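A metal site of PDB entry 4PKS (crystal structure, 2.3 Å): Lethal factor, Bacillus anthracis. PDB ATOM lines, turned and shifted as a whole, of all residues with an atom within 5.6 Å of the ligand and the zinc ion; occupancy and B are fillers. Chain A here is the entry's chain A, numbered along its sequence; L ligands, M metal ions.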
ATOM      1  N   ASP A  67      -0.358 -25.959 -14.845  1.00  0.00           N
ATOM      2  CA  ASP A  67       0.591 -25.725 -13.760  1.00  0.00           C
ATOM      3  C   ASP A  67       1.170 -24.310 -13.771  1.00  0.00           C
ATOM      4  O   ASP A  67       1.549 -23.799 -12.716  1.00  0.00           O
ATOM      5  CB  ASP A  67       1.740 -26.739 -13.848  1.00  0.00           C
ATOM      6  CG  ASP A  67       1.339 -28.119 -13.366  1.00  0.00           C
ATOM      7  OD1 ASP A  67       0.170 -28.310 -12.990  1.00  0.00           O
ATOM      8  OD2 ASP A  67       2.209 -29.017 -13.357  1.00  0.00           O
ATOM      9  N   PHE A  68       1.239 -23.700 -14.945  1.00  0.00           N
ATOM     10  CA  PHE A  68       1.974 -22.449 -15.090  1.00  0.00           C
ATOM     11  C   PHE A  68       1.129 -21.210 -15.383  1.00  0.00           C
ATOM     12  O   PHE A  68       1.638 -20.219 -15.897  1.00  0.00           O
ATOM     13  CB  PHE A  68       3.020 -22.589 -16.196  1.00  0.00           C
ATOM     14  CG  PHE A  68       4.326 -23.164 -15.730  1.00  0.00           C
ATOM     15  CD1 PHE A  68       4.353 -24.101 -14.707  1.00  0.00           C
ATOM     16  CD2 PHE A  68       5.518 -22.760 -16.291  1.00  0.00           C
ATOM     17  CE1 PHE A  68       5.548 -24.642 -14.278  1.00  0.00           C
ATOM     18  CE2 PHE A  68       6.719 -23.277 -15.865  1.00  0.00           C
ATOM     19  CZ  PHE A  68       6.728 -24.224 -14.851  1.00  0.00           C
ATOM     20  N   VAL A 392      10.407 -18.755 -18.266  1.00  0.00           N
ATOM     21  CA  VAL A 392       9.710 -19.270 -17.091  1.00  0.00           C
ATOM     22  C   VAL A 392       9.888 -18.352 -15.886  1.00  0.00           C
ATOM     23  O   VAL A 392      10.995 -17.909 -15.590  1.00  0.00           O
ATOM     24  CB  VAL A 392      10.213 -20.690 -16.721  1.00  0.00           C
ATOM     25  CG1 VAL A 392       9.646 -21.139 -15.379  1.00  0.00           C
ATOM     26  CG2 VAL A 392       9.852 -21.683 -17.816  1.00  0.00           C
ATOM     27  N   SER A 394       9.154 -18.553 -11.746  1.00  0.00           N
ATOM     28  CA  SER A 394       8.830 -19.466 -10.658  1.00  0.00           C
ATOM     29  C   SER A 394       9.657 -19.128  -9.427  1.00  0.00           C
ATOM     30  O   SER A 394      10.420 -18.162  -9.437  1.00  0.00           O
ATOM     31  CB  SER A 394       9.062 -20.918 -11.094  1.00  0.00           C
ATOM     32  OG  SER A 394      10.352 -21.081 -11.676  1.00  0.00           O
ATOM     33  N   LYS A 395       9.505 -19.927  -8.373  1.00  0.00           N
ATOM     34  CA  LYS A 395      10.304 -19.752  -7.166  1.00  0.00           C
ATOM     35  C   LYS A 395      11.778 -19.953  -7.468  1.00  0.00           C
ATOM     36  O   LYS A 395      12.622 -19.146  -7.048  1.00  0.00           O
ATOM     37  CB  LYS A 395       9.839 -20.733  -6.079  1.00  0.00           C
ATOM     38  CG  LYS A 395      10.889 -21.068  -5.029  1.00  0.00           C
ATOM     39  CD  LYS A 395      11.261 -19.852  -4.183  1.00  0.00           C
ATOM     40  CE  LYS A 395      10.070 -19.365  -3.380  1.00  0.00           C
ATOM     41  NZ  LYS A 395      10.437 -18.169  -2.560  1.00  0.00           N
ATOM     42  N   GLY A 396      12.088 -21.002  -8.204  1.00  0.00           N
ATOM     43  CA  GLY A 396      13.465 -21.333  -8.514  1.00  0.00           C
ATOM     44  C   GLY A 396      13.627 -21.853  -9.929  1.00  0.00           C
ATOM     45  O   GLY A 396      12.664 -22.328 -10.543  1.00  0.00           O
ATOM     46  N   LEU A 397      14.841 -21.763 -10.452  1.00  0.00           N
ATOM     47  CA  LEU A 397      15.129 -22.215 -11.803  1.00  0.00           C
ATOM     48  C   LEU A 397      16.602 -22.577 -11.963  1.00  0.00           C
ATOM     49  O   LEU A 397      17.466 -22.034 -11.280  1.00  0.00           O
ATOM     50  CB  LEU A 397      14.741 -21.141 -12.816  1.00  0.00           C
ATOM     51  CG  LEU A 397      14.672 -21.577 -14.279  1.00  0.00           C
ATOM     52  CD1 LEU A 397      13.613 -22.654 -14.446  1.00  0.00           C
ATOM     53  CD2 LEU A 397      14.403 -20.394 -15.194  1.00  0.00           C
ATOM     54  N   TYR A 398      16.883 -23.510 -12.874  1.00  0.00           N
ATOM     55  CA  TYR A 398      18.251 -23.794 -13.284  1.00  0.00           C
ATOM     56  C   TYR A 398      18.398 -23.670 -14.801  1.00  0.00           C
ATOM     57  O   TYR A 398      17.601 -24.228 -15.548  1.00  0.00           O
ATOM     58  CB  TYR A 398      18.691 -25.180 -12.824  1.00  0.00           C
ATOM     59  CG  TYR A 398      20.092 -25.510 -13.284  1.00  0.00           C
ATOM     60  CD1 TYR A 398      21.195 -24.926 -12.678  1.00  0.00           C
ATOM     61  CD2 TYR A 398      20.308 -26.377 -14.347  1.00  0.00           C
ATOM     62  CE1 TYR A 398      22.475 -25.217 -13.105  1.00  0.00           C
ATOM     63  CE2 TYR A 398      21.587 -26.661 -14.789  1.00  0.00           C
ATOM     64  CZ  TYR A 398      22.659 -26.083 -14.159  1.00  0.00           C
ATOM     65  OH  TYR A 398      23.939 -26.373 -14.586  1.00  0.00           O
ATOM     66  N   GLY A 413       6.776 -21.348  -3.744  1.00  0.00           N
ATOM     67  CA  GLY A 413       6.786 -22.534  -4.586  1.00  0.00           C
ATOM     68  C   GLY A 413       5.643 -23.475  -4.268  1.00  0.00           C
ATOM     69  O   GLY A 413       5.352 -23.744  -3.104  1.00  0.00           O
ATOM     70  N   VAL A 414       4.976 -23.964  -5.312  1.00  0.00           N
ATOM     71  CA  VAL A 414       3.853 -24.873  -5.144  1.00  0.00           C
ATOM     72  C   VAL A 414       4.301 -26.184  -4.505  1.00  0.00           C
ATOM     73  O   VAL A 414       5.214 -26.842  -5.013  1.00  0.00           O
ATOM     74  CB  VAL A 414       3.156 -25.178  -6.480  1.00  0.00           C
ATOM     75  CG1 VAL A 414       1.933 -26.053  -6.250  1.00  0.00           C
ATOM     76  CG2 VAL A 414       2.767 -23.882  -7.177  1.00  0.00           C
ATOM     77  N   GLU A 415       3.660 -26.540  -3.402  1.00  0.00           N
ATOM     78  CA  GLU A 415       4.019 -27.736  -2.620  1.00  0.00           C
ATOM     79  C   GLU A 415       5.493 -27.703  -2.242  1.00  0.00           C
ATOM     80  O   GLU A 415       6.238 -28.655  -2.490  1.00  0.00           O
ATOM     81  CB  GLU A 415       3.694 -29.005  -3.403  1.00  0.00           C
ATOM     82  CG  GLU A 415       2.264 -29.493  -3.204  1.00  0.00           C
ATOM     83  CD  GLU A 415       1.656 -30.084  -4.458  1.00  0.00           C
ATOM     84  OE1 GLU A 415       1.142 -29.308  -5.290  1.00  0.00           O
ATOM     85  OE2 GLU A 415       1.711 -31.327  -4.611  1.00  0.00           O
ATOM     86  N   LEU A 416       5.904 -26.585  -1.647  1.00  0.00           N
ATOM     87  CA  LEU A 416       7.292 -26.378  -1.240  1.00  0.00           C
ATOM     88  C   LEU A 416       7.326 -25.665   0.109  1.00  0.00           C
ATOM     89  O   LEU A 416       6.739 -24.588   0.261  1.00  0.00           O
ATOM     90  CB  LEU A 416       8.045 -25.574  -2.292  1.00  0.00           C
ATOM     91  CG  LEU A 416       9.558 -25.415  -2.115  1.00  0.00           C
ATOM     92  CD1 LEU A 416      10.247 -26.759  -2.296  1.00  0.00           C
ATOM     93  CD2 LEU A 416      10.095 -24.399  -3.099  1.00  0.00           C
ATOM     94  N   GLU A 421      14.673 -25.580   0.470  1.00  0.00           N
ATOM     95  CA  GLU A 421      14.261 -26.794  -0.231  1.00  0.00           C
ATOM     96  C   GLU A 421      14.193 -26.552  -1.733  1.00  0.00           C
ATOM     97  O   GLU A 421      14.499 -27.431  -2.532  1.00  0.00           O
ATOM     98  CB  GLU A 421      12.917 -27.302   0.291  1.00  0.00           C
ATOM     99  CG  GLU A 421      12.966 -27.805   1.724  1.00  0.00           C
ATOM    100  CD  GLU A 421      11.742 -28.606   2.100  1.00  0.00           C
ATOM    101  OE1 GLU A 421      10.720 -28.500   1.381  1.00  0.00           O
ATOM    102  OE2 GLU A 421      11.802 -29.361   3.094  1.00  0.00           O
ATOM    103  N   GLY A 422      13.782 -25.343  -2.116  1.00  0.00           N
ATOM    104  CA  GLY A 422      13.732 -24.976  -3.515  1.00  0.00           C
ATOM    105  C   GLY A 422      15.124 -24.938  -4.117  1.00  0.00           C
ATOM    106  O   GLY A 422      15.343 -25.438  -5.222  1.00  0.00           O
ATOM    107  N   HIS A 425      16.514 -28.370  -4.769  1.00  0.00           N
ATOM    108  CA  HIS A 425      15.913 -28.872  -5.995  1.00  0.00           C
ATOM    109  C   HIS A 425      16.653 -28.369  -7.232  1.00  0.00           C
ATOM    110  O   HIS A 425      16.981 -29.145  -8.129  1.00  0.00           O
ATOM    111  CB  HIS A 425      14.434 -28.460  -6.044  1.00  0.00           C
ATOM    112  CG  HIS A 425      13.749 -28.762  -7.350  1.00  0.00           C
ATOM    113  ND1 HIS A 425      12.855 -29.800  -7.492  1.00  0.00           N
ATOM    114  CD2 HIS A 425      13.788 -28.135  -8.540  1.00  0.00           C
ATOM    115  CE1 HIS A 425      12.386 -29.797  -8.726  1.00  0.00           C
ATOM    116  NE2 HIS A 425      12.937 -28.808  -9.386  1.00  0.00           N
ATOM    117  N   GLU A 426      16.912 -27.067  -7.271  1.00  0.00           N
ATOM    118  CA  GLU A 426      17.644 -26.482  -8.402  1.00  0.00           C
ATOM    119  C   GLU A 426      19.061 -27.043  -8.482  1.00  0.00           C
ATOM    120  O   GLU A 426      19.606 -27.208  -9.567  1.00  0.00           O
ATOM    121  CB  GLU A 426      17.701 -24.949  -8.285  1.00  0.00           C
ATOM    122  CG  GLU A 426      16.375 -24.271  -7.959  1.00  0.00           C
ATOM    123  CD  GLU A 426      15.269 -24.598  -8.955  1.00  0.00           C
ATOM    124  OE1 GLU A 426      14.086 -24.544  -8.557  1.00  0.00           O
ATOM    125  OE2 GLU A 426      15.578 -24.892 -10.127  1.00  0.00           O
ATOM    126  N   HIS A 429      19.209 -30.164 -10.439  1.00  0.00           N
ATOM    127  CA  HIS A 429      19.371 -29.936 -11.877  1.00  0.00           C
ATOM    128  C   HIS A 429      20.835 -29.749 -12.252  1.00  0.00           C
ATOM    129  O   HIS A 429      21.270 -30.227 -13.304  1.00  0.00           O
ATOM    130  CB  HIS A 429      18.575 -28.697 -12.322  1.00  0.00           C
ATOM    131  CG  HIS A 429      17.090 -28.896 -12.324  1.00  0.00           C
ATOM    132  ND1 HIS A 429      16.484 -29.972 -12.930  1.00  0.00           N
ATOM    133  CD2 HIS A 429      16.087 -28.138 -11.810  1.00  0.00           C
ATOM    134  CE1 HIS A 429      15.172 -29.873 -12.787  1.00  0.00           C
ATOM    135  NE2 HIS A 429      14.907 -28.768 -12.113  1.00  0.00           N
ATOM    136  N   TYR A 467       4.349 -33.213  -9.054  1.00  0.00           N
ATOM    137  CA  TYR A 467       5.076 -32.407 -10.023  1.00  0.00           C
ATOM    138  C   TYR A 467       6.284 -33.163 -10.584  1.00  0.00           C
ATOM    139  O   TYR A 467       6.756 -32.863 -11.689  1.00  0.00           O
ATOM    140  CB  TYR A 467       5.522 -31.084  -9.418  1.00  0.00           C
ATOM    141  CG  TYR A 467       6.330 -30.254 -10.377  1.00  0.00           C
ATOM    142  CD1 TYR A 467       5.742 -29.713 -11.507  1.00  0.00           C
ATOM    143  CD2 TYR A 467       7.683 -30.053 -10.181  1.00  0.00           C
ATOM    144  CE1 TYR A 467       6.470 -28.965 -12.406  1.00  0.00           C
ATOM    145  CE2 TYR A 467       8.433 -29.304 -11.069  1.00  0.00           C
ATOM    146  CZ  TYR A 467       7.822 -28.768 -12.181  1.00  0.00           C
ATOM    147  OH  TYR A 467       8.558 -28.025 -13.070  1.00  0.00           O
ATOM    148  N   GLU A 474      12.747 -32.981 -13.957  1.00  0.00           N
ATOM    149  CA  GLU A 474      12.005 -32.578 -12.775  1.00  0.00           C
ATOM    150  C   GLU A 474      11.867 -33.735 -11.786  1.00  0.00           C
ATOM    151  O   GLU A 474      11.895 -33.531 -10.579  1.00  0.00           O
ATOM    152  CB  GLU A 474      10.615 -32.047 -13.161  1.00  0.00           C
ATOM    153  CG  GLU A 474      10.586 -30.606 -13.690  1.00  0.00           C
ATOM    154  CD  GLU A 474      11.596 -29.677 -13.025  1.00  0.00           C
ATOM    155  OE1 GLU A 474      11.724 -29.699 -11.775  1.00  0.00           O
ATOM    156  OE2 GLU A 474      12.244 -28.914 -13.760  1.00  0.00           O
ATOM    157  N   ALA A 477      15.242 -34.029 -10.062  1.00  0.00           N
ATOM    158  CA  ALA A 477      15.471 -32.941  -9.116  1.00  0.00           C
ATOM    159  C   ALA A 477      14.594 -33.067  -7.886  1.00  0.00           C
ATOM    160  O   ALA A 477      15.022 -32.743  -6.777  1.00  0.00           O
ATOM    161  CB  ALA A 477      15.232 -31.602  -9.792  1.00  0.00           C
ATOM    162  N   GLU A 478      13.362 -33.538  -8.069  1.00  0.00           N
ATOM    163  CA  GLU A 478      12.448 -33.780  -6.963  1.00  0.00           C
ATOM    164  C   GLU A 478      12.961 -34.909  -6.083  1.00  0.00           C
ATOM    165  O   GLU A 478      12.958 -34.801  -4.856  1.00  0.00           O
ATOM    166  CB  GLU A 478      11.050 -34.098  -7.475  1.00  0.00           C
ATOM    167  CG  GLU A 478      10.240 -32.875  -7.875  1.00  0.00           C
ATOM    168  CD  GLU A 478       9.917 -31.992  -6.683  1.00  0.00           C
ATOM    169  OE1 GLU A 478       8.847 -32.188  -6.066  1.00  0.00           O
ATOM    170  OE2 GLU A 478      10.735 -31.100  -6.358  1.00  0.00           O
ATOM    171  N   ARG A 481      15.839 -33.715  -4.095  1.00  0.00           N
ATOM    172  CA  ARG A 481      15.399 -32.854  -3.011  1.00  0.00           C
ATOM    173  C   ARG A 481      14.958 -33.669  -1.805  1.00  0.00           C
ATOM    174  O   ARG A 481      15.397 -33.427  -0.685  1.00  0.00           O
ATOM    175  CB  ARG A 481      14.244 -31.949  -3.468  1.00  0.00           C
ATOM    176  CG  ARG A 481      13.645 -31.106  -2.346  1.00  0.00           C
ATOM    177  CD  ARG A 481      12.584 -30.140  -2.833  1.00  0.00           C
ATOM    178  NE  ARG A 481      11.404 -30.814  -3.378  1.00  0.00           N
ATOM    179  CZ  ARG A 481      10.389 -31.244  -2.644  1.00  0.00           C
ATOM    180  NH1 ARG A 481      10.394 -31.086  -1.329  1.00  0.00           N
ATOM    181  NH2 ARG A 481       9.356 -31.850  -3.231  1.00  0.00           N
HETATM  182  O1  LIG L   1      11.042 -26.557 -11.694  1.00  0.00           O
HETATM  183  C1  LIG L   1       9.372 -24.357 -12.550  1.00  0.00           C
HETATM  184  C2  LIG L   1       8.211 -25.913 -10.467  1.00  0.00           C
HETATM  185  C3  LIG L   1       6.735 -25.584 -10.499  1.00  0.00           C
HETATM  186  C4  LIG L   1       6.256 -24.371 -10.970  1.00  0.00           C
HETATM  187  C5  LIG L   1       4.888 -24.158 -10.972  1.00  0.00           C
HETATM  188  C6  LIG L   1       4.026 -25.145 -10.501  1.00  0.00           C
HETATM  189  C7  LIG L   1       5.841 -26.544 -10.047  1.00  0.00           C
HETATM  190  C8  LIG L   1       9.799 -25.192  -7.748  1.00  0.00           C
HETATM  191  C9  LIG L   1       9.019 -26.184  -7.171  1.00  0.00           C
HETATM  192  C10 LIG L   1       9.589 -27.116  -6.304  1.00  0.00           C
HETATM  193  C11 LIG L   1      11.205 -25.423 -11.285  1.00  0.00           C
HETATM  194  C12 LIG L   1      10.058 -24.450 -11.188  1.00  0.00           C
HETATM  195  N1  LIG L   1      12.404 -24.980 -10.918  1.00  0.00           N
HETATM  196  O2  LIG L   1      13.549 -25.658 -11.346  1.00  0.00           O
HETATM  197  N2  LIG L   1       9.114 -24.806 -10.131  1.00  0.00           N
HETATM  198  S1  LIG L   1       9.134 -24.145  -8.745  1.00  0.00           S
HETATM  199  O3  LIG L   1       7.805 -23.821  -8.291  1.00  0.00           O
HETATM  200  O4  LIG L   1       9.914 -22.938  -8.792  1.00  0.00           O
HETATM  201  N3  LIG L   1       4.520 -26.313 -10.051  1.00  0.00           N
HETATM  202  C13 LIG L   1      10.947 -27.043  -6.016  1.00  0.00           C
HETATM  203  C14 LIG L   1      11.732 -26.047  -6.585  1.00  0.00           C
HETATM  204  C15 LIG L   1      11.162 -25.114  -7.452  1.00  0.00           C
HETATM  205  F1  LIG L   1      11.488 -27.939  -5.176  1.00  0.00           F
HETATM  206  C16 LIG L   1       8.745 -28.187  -5.680  1.00  0.00           C
HETATM  207 ZN    ZN M   1      12.895 -27.905 -11.625  1.00  0.00          ZN
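The zinc ion is bound by the side-chain carboxylate (OE1) of Glu 474 (2.1 Å), a ring nitrogen (NE2) of His 429 (2.2 Å), an oxygen (O1) of the ligand (2.3 Å), an oxygen (O2) of the ligand (2.4 Å), a ring nitrogen (NE2) of His 425 (2.4 Å) and the side-chain carboxylate (OE2) of Glu 474 (2.4 Å).
The backbone NH (N) of Lys 395 lies within hydrogen-bond range of an oxygen (O4) of the ligand (3.1 Å). A nitrogen (N1) of the ligand is in hydrogen-bond range of the backbone carbonyl oxygen (O) of Gly 396 (2.7 Å). The backbone NH (N) of Gly 396 is in hydrogen-bond range of an oxygen (O4) of the ligand (3.0 Å). OH of Tyr 467 lies close to O1 of the ligand. A nitrogen (N1) of the ligand is in hydrogen-bond range of the side-chain carboxylate (OE1) of Glu 426, at 2.9 Å. OG of Ser 394 lies close to O4 of the ligand, at 3.5 Å.
N of Tyr 398 sits at hydrogen-bond distance from OE2 of Glu 426, at 3.3 Å. The side-chain carboxylate (OE1) of Glu 478 is in salt-bridge range of the guanidinium group (NH2) of Arg 481, at 2.9 Å. The side-chain carboxylate of Glu 478 lies within hydrogen-bond range of a ring nitrogen (ND1) of His 425 (2.7 Å). The side-chain hydroxyl (OG) of Ser 394 sits at hydrogen-bond distance from the backbone carbonyl oxygen (O) of Gly 396 (2.9 Å). OE2 of Glu 426 sits close to N of Leu 397, 3.2 Å away. The side-chain carboxylate (OE1) of Glu 421 is in salt-bridge range of the guanidinium group (NH1) of Arg 481.
Three residues have an atom within 4 Å of the zinc ion: His 425, His 429 and Glu 474.
The side-chain carboxylate (OE2) of Glu 478 lies close to a fluorine (F1) of the ligand (3.5 Å). F1 of the ligand lies close to NE of Arg 481 (3.4 Å). Merely in contact with the ligand: Asp 67 (3.6 Å), Phe 68 (3.4 Å), Leu 397 (3.8 Å), Val 414 (3.8 Å), Leu 416 (3.4 Å) and Gly 422 (3.8 Å). Hydrophobic or aromatic side chains that line the ligand: Phe 68, Val 414, Leu 416, His 425, His 429 and Tyr 467. Within 4 Å of the ligand: Asp 67, Phe 68, Ser 394, Lys 395, Gly 396, Leu 397, Val 414, Leu 416, Gly 422, His 425, Glu 426, His 429, Tyr 467, Glu 474, Glu 478 and Arg 481.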
